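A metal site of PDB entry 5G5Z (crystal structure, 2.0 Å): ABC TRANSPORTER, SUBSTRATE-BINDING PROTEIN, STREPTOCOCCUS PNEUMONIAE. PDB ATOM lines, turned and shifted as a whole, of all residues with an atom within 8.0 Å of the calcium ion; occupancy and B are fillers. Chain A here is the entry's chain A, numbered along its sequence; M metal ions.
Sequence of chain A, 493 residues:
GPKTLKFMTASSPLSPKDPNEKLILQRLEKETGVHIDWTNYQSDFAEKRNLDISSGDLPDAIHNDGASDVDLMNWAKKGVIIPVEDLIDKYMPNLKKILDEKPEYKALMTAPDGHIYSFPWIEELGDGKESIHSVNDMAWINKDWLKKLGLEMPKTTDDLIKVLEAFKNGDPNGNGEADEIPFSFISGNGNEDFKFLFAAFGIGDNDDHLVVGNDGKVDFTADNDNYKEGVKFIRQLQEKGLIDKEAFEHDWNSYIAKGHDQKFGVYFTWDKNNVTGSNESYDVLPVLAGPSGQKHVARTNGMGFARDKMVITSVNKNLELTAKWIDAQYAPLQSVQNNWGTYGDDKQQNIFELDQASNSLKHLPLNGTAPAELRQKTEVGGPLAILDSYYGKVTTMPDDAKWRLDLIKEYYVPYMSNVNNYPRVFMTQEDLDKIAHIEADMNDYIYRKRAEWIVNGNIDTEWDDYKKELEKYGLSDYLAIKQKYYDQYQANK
OD2 of Asp 179 is in salt-bridge range of NZ of Lys 263, 2.8 Å away. OD1 of Asp 171 lies close to N of Gly 174 (3.3 Å). N of Gly 176 lies within hydrogen-bond range of OD2 of Asp 171 (2.7 Å).
The backbone carbonyl oxygen (O) of Glu 177 binds the calcium ion (2.2 Å). OD1 of Asp 179 is bound to the calcium ion (2.4 Å). OD1 of Asn 173 is bound to the calcium ion (2.4 Å). The side-chain carboxylate (OD1) of Asp 171 binds the calcium ion (2.4 Å). The side-chain amide oxygen (OD1) of Asn 175 binds the calcium ion (2.5 Å). The calcium ion is bound by OE2 of Glu 180 (2.5 Å). OE1 of Glu 180 is bound to the calcium ion, at 2.6 Å.
Six residues have an atom within 4 Å of the calcium ion: Asp 171, Asn 173, Asn 175, Glu 177, Asp 179 and Glu 180.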
ATOM      1  N   TRP A 145      23.228 -29.576  -4.324  1.00  0.00           N
ATOM      2  CA  TRP A 145      22.169 -29.181  -5.244  1.00  0.00           C
ATOM      3  C   TRP A 145      22.657 -29.153  -6.691  1.00  0.00           C
ATOM      4  O   TRP A 145      21.909 -29.525  -7.598  1.00  0.00           O
ATOM      5  CB  TRP A 145      21.594 -27.817  -4.871  1.00  0.00           C
ATOM      6  CG  TRP A 145      20.780 -27.877  -3.646  1.00  0.00           C
ATOM      7  CD1 TRP A 145      20.567 -28.966  -2.862  1.00  0.00           C
ATOM      8  CD2 TRP A 145      20.058 -26.801  -3.050  1.00  0.00           C
ATOM      9  NE1 TRP A 145      19.760 -28.644  -1.814  1.00  0.00           N
ATOM     10  CE2 TRP A 145      19.435 -27.309  -1.895  1.00  0.00           C
ATOM     11  CE3 TRP A 145      19.892 -25.454  -3.371  1.00  0.00           C
ATOM     12  CZ2 TRP A 145      18.626 -26.527  -1.062  1.00  0.00           C
ATOM     13  CZ3 TRP A 145      19.099 -24.668  -2.534  1.00  0.00           C
ATOM     14  CH2 TRP A 145      18.482 -25.210  -1.388  1.00  0.00           C
ATOM     15  N   PHE A 167      17.836 -23.705  -8.818  1.00  0.00           N
ATOM     16  CA  PHE A 167      17.563 -23.918  -7.405  1.00  0.00           C
ATOM     17  C   PHE A 167      16.123 -23.566  -7.080  1.00  0.00           C
ATOM     18  O   PHE A 167      15.420 -24.315  -6.389  1.00  0.00           O
ATOM     19  CB  PHE A 167      18.509 -23.043  -6.562  1.00  0.00           C
ATOM     20  CG  PHE A 167      19.944 -23.484  -6.575  1.00  0.00           C
ATOM     21  CD1 PHE A 167      20.325 -24.694  -7.126  1.00  0.00           C
ATOM     22  CD2 PHE A 167      20.923 -22.682  -5.995  1.00  0.00           C
ATOM     23  CE1 PHE A 167      21.670 -25.088  -7.123  1.00  0.00           C
ATOM     24  CE2 PHE A 167      22.241 -23.070  -5.988  1.00  0.00           C
ATOM     25  CZ  PHE A 167      22.619 -24.287  -6.545  1.00  0.00           C
ATOM     26  N   LYS A 168      15.663 -22.419  -7.584  1.00  0.00           N
ATOM     27  CA  LYS A 168      14.327 -21.924  -7.279  1.00  0.00           C
ATOM     28  C   LYS A 168      13.246 -22.881  -7.746  1.00  0.00           C
ATOM     29  O   LYS A 168      12.310 -23.192  -7.006  1.00  0.00           O
ATOM     30  CB  LYS A 168      14.146 -20.545  -7.916  1.00  0.00           C
ATOM     31  CG  LYS A 168      12.821 -19.903  -7.627  1.00  0.00           C
ATOM     32  CD  LYS A 168      12.654 -18.618  -8.415  1.00  0.00           C
ATOM     33  CE  LYS A 168      11.253 -18.052  -8.277  1.00  0.00           C
ATOM     34  NZ  LYS A 168      10.859 -17.837  -6.834  1.00  0.00           N
ATOM     35  N   ASN A 169      13.358 -23.382  -8.992  1.00  0.00           N
ATOM     36  CA  ASN A 169      12.286 -24.135  -9.637  1.00  0.00           C
ATOM     37  C   ASN A 169      12.519 -25.639  -9.704  1.00  0.00           C
ATOM     38  O   ASN A 169      11.570 -26.369 -10.046  1.00  0.00           O
ATOM     39  CB  ASN A 169      12.060 -23.602 -11.069  1.00  0.00           C
ATOM     40  CG  ASN A 169      11.757 -22.111 -11.101  1.00  0.00           C
ATOM     41  OD1 ASN A 169      10.908 -21.596 -10.356  1.00  0.00           O
ATOM     42  ND2 ASN A 169      12.467 -21.390 -11.953  1.00  0.00           N
ATOM     43  N   GLY A 170      13.709 -26.136  -9.389  1.00  0.00           N
ATOM     44  CA  GLY A 170      14.040 -27.529  -9.626  1.00  0.00           C
ATOM     45  C   GLY A 170      13.837 -28.516  -8.488  1.00  0.00           C
ATOM     46  O   GLY A 170      14.018 -29.717  -8.709  1.00  0.00           O
ATOM     47  N   ASP A 171      13.456 -28.062  -7.296  1.00  0.00           N
ATOM     48  CA  ASP A 171      13.317 -28.923  -6.124  1.00  0.00           C
ATOM     49  C   ASP A 171      14.541 -29.806  -5.900  1.00  0.00           C
ATOM     50  O   ASP A 171      14.428 -31.036  -5.820  1.00  0.00           O
ATOM     51  CB  ASP A 171      12.048 -29.776  -6.236  1.00  0.00           C
ATOM     52  CG  ASP A 171      11.753 -30.576  -4.974  1.00  0.00           C
ATOM     53  OD1 ASP A 171      12.197 -30.147  -3.878  1.00  0.00           O
ATOM     54  OD2 ASP A 171      11.070 -31.635  -5.060  1.00  0.00           O
ATOM     55  N   PRO A 172      15.735 -29.223  -5.760  1.00  0.00           N
ATOM     56  CA  PRO A 172      16.946 -30.055  -5.605  1.00  0.00           C
ATOM     57  C   PRO A 172      17.076 -30.712  -4.227  1.00  0.00           C
ATOM     58  O   PRO A 172      17.948 -31.582  -4.076  1.00  0.00           O
ATOM     59  CB  PRO A 172      18.093 -29.061  -5.861  1.00  0.00           C
ATOM     60  CG  PRO A 172      17.533 -27.749  -5.401  1.00  0.00           C
ATOM     61  CD  PRO A 172      16.082 -27.786  -5.828  1.00  0.00           C
ATOM     62  N   ASN A 173      16.272 -30.345  -3.234  1.00  0.00           N
ATOM     63  CA  ASN A 173      16.251 -31.143  -2.010  1.00  0.00           C
ATOM     64  C   ASN A 173      15.169 -32.221  -2.033  1.00  0.00           C
ATOM     65  O   ASN A 173      14.948 -32.870  -1.010  1.00  0.00           O
ATOM     66  CB  ASN A 173      16.131 -30.252  -0.752  1.00  0.00           C
ATOM     67  CG  ASN A 173      14.761 -29.608  -0.575  1.00  0.00           C
ATOM     68  OD1 ASN A 173      13.802 -29.903  -1.291  1.00  0.00           O
ATOM     69  ND2 ASN A 173      14.660 -28.719   0.406  1.00  0.00           N
ATOM     70  N   GLY A 174      14.494 -32.391  -3.174  1.00  0.00           N
ATOM     71  CA  GLY A 174      13.669 -33.552  -3.465  1.00  0.00           C
ATOM     72  C   GLY A 174      12.352 -33.675  -2.718  1.00  0.00           C
ATOM     73  O   GLY A 174      11.624 -34.654  -2.943  1.00  0.00           O
ATOM     74  N   ASN A 175      12.014 -32.727  -1.849  1.00  0.00           N
ATOM     75  CA  ASN A 175      10.854 -32.862  -0.965  1.00  0.00           C
ATOM     76  C   ASN A 175       9.568 -32.316  -1.567  1.00  0.00           C
ATOM     77  O   ASN A 175       8.637 -31.996  -0.815  1.00  0.00           O
ATOM     78  CB  ASN A 175      11.137 -32.180   0.382  1.00  0.00           C
ATOM     79  CG  ASN A 175      11.395 -30.677   0.243  1.00  0.00           C
ATOM     80  OD1 ASN A 175      11.098 -30.063  -0.792  1.00  0.00           O
ATOM     81  ND2 ASN A 175      11.944 -30.086   1.297  1.00  0.00           N
ATOM     82  N   GLY A 176       9.498 -32.185  -2.883  1.00  0.00           N
ATOM     83  CA  GLY A 176       8.303 -31.716  -3.546  1.00  0.00           C
ATOM     84  C   GLY A 176       7.743 -30.394  -3.050  1.00  0.00           C
ATOM     85  O   GLY A 176       6.525 -30.199  -3.065  1.00  0.00           O
ATOM     86  N   GLU A 177       8.599 -29.476  -2.601  1.00  0.00           N
ATOM     87  CA  GLU A 177       8.132 -28.147  -2.232  1.00  0.00           C
ATOM     88  C   GLU A 177       9.157 -27.096  -2.614  1.00  0.00           C
ATOM     89  O   GLU A 177      10.359 -27.364  -2.698  1.00  0.00           O
ATOM     90  CB  GLU A 177       7.818 -28.065  -0.731  1.00  0.00           C
ATOM     91  CG  GLU A 177       6.387 -28.446  -0.400  1.00  0.00           C
ATOM     92  CD  GLU A 177       6.083 -28.375   1.093  1.00  0.00           C
ATOM     93  OE1 GLU A 177       7.042 -28.411   1.892  1.00  0.00           O
ATOM     94  OE2 GLU A 177       4.895 -28.283   1.455  1.00  0.00           O
ATOM     95  N   ALA A 178       8.662 -25.883  -2.862  1.00  0.00           N
ATOM     96  CA  ALA A 178       9.508 -24.739  -3.213  1.00  0.00           C
ATOM     97  C   ALA A 178      10.053 -24.034  -1.972  1.00  0.00           C
ATOM     98  O   ALA A 178       9.858 -22.840  -1.784  1.00  0.00           O
ATOM     99  CB  ALA A 178       8.717 -23.769  -4.088  1.00  0.00           C
ATOM    100  N   ASP A 179      10.739 -24.787  -1.115  1.00  0.00           N
ATOM    101  CA  ASP A 179      11.380 -24.223   0.059  1.00  0.00           C
ATOM    102  C   ASP A 179      12.778 -23.723  -0.237  1.00  0.00           C
ATOM    103  O   ASP A 179      13.381 -23.068   0.624  1.00  0.00           O
ATOM    104  CB  ASP A 179      11.440 -25.266   1.183  1.00  0.00           C
ATOM    105  CG  ASP A 179      12.154 -26.539   0.756  1.00  0.00           C
ATOM    106  OD1 ASP A 179      12.214 -26.814  -0.460  1.00  0.00           O
ATOM    107  OD2 ASP A 179      12.653 -27.259   1.639  1.00  0.00           O
ATOM    108  N   GLU A 180      13.317 -24.015  -1.413  1.00  0.00           N
ATOM    109  CA  GLU A 180      14.664 -23.564  -1.726  1.00  0.00           C
ATOM    110  C   GLU A 180      14.700 -22.044  -1.696  1.00  0.00           C
ATOM    111  O   GLU A 180      13.844 -21.371  -2.278  1.00  0.00           O
ATOM    112  CB  GLU A 180      15.100 -24.073  -3.099  1.00  0.00           C
ATOM    113  CG  GLU A 180      15.493 -25.563  -3.154  1.00  0.00           C
ATOM    114  CD  GLU A 180      14.301 -26.526  -3.059  1.00  0.00           C
ATOM    115  OE1 GLU A 180      13.138 -26.070  -2.972  1.00  0.00           O
ATOM    116  OE2 GLU A 180      14.534 -27.755  -3.079  1.00  0.00           O
ATOM    117  N   ILE A 181      15.694 -21.500  -0.998  1.00  0.00           N
ATOM    118  CA  ILE A 181      16.019 -20.089  -1.026  1.00  0.00           C
ATOM    119  C   ILE A 181      17.294 -19.928  -1.863  1.00  0.00           C
ATOM    120  O   ILE A 181      18.379 -20.303  -1.406  1.00  0.00           O
ATOM    121  CB  ILE A 181      16.216 -19.530   0.388  1.00  0.00           C
ATOM    122  CG1 ILE A 181      14.940 -19.662   1.222  1.00  0.00           C
ATOM    123  CG2 ILE A 181      16.697 -18.093   0.327  1.00  0.00           C
ATOM    124  CD1 ILE A 181      15.186 -19.383   2.672  1.00  0.00           C
ATOM    125  N   LYS A 263      18.658 -24.681   3.538  1.00  0.00           N
ATOM    126  CA  LYS A 263      17.690 -24.041   2.644  1.00  0.00           C
ATOM    127  C   LYS A 263      18.339 -23.127   1.609  1.00  0.00           C
ATOM    128  O   LYS A 263      17.658 -22.682   0.679  1.00  0.00           O
ATOM    129  CB  LYS A 263      16.678 -23.194   3.437  1.00  0.00           C
ATOM    130  CG  LYS A 263      15.886 -23.912   4.527  1.00  0.00           C
ATOM    131  CD  LYS A 263      14.885 -24.860   3.888  1.00  0.00           C
ATOM    132  CE  LYS A 263      13.972 -25.493   4.914  1.00  0.00           C
ATOM    133  NZ  LYS A 263      13.190 -26.591   4.262  1.00  0.00           N
HETATM  134 CA    CA M   1      12.221 -28.384  -2.249  1.00  0.00          CA
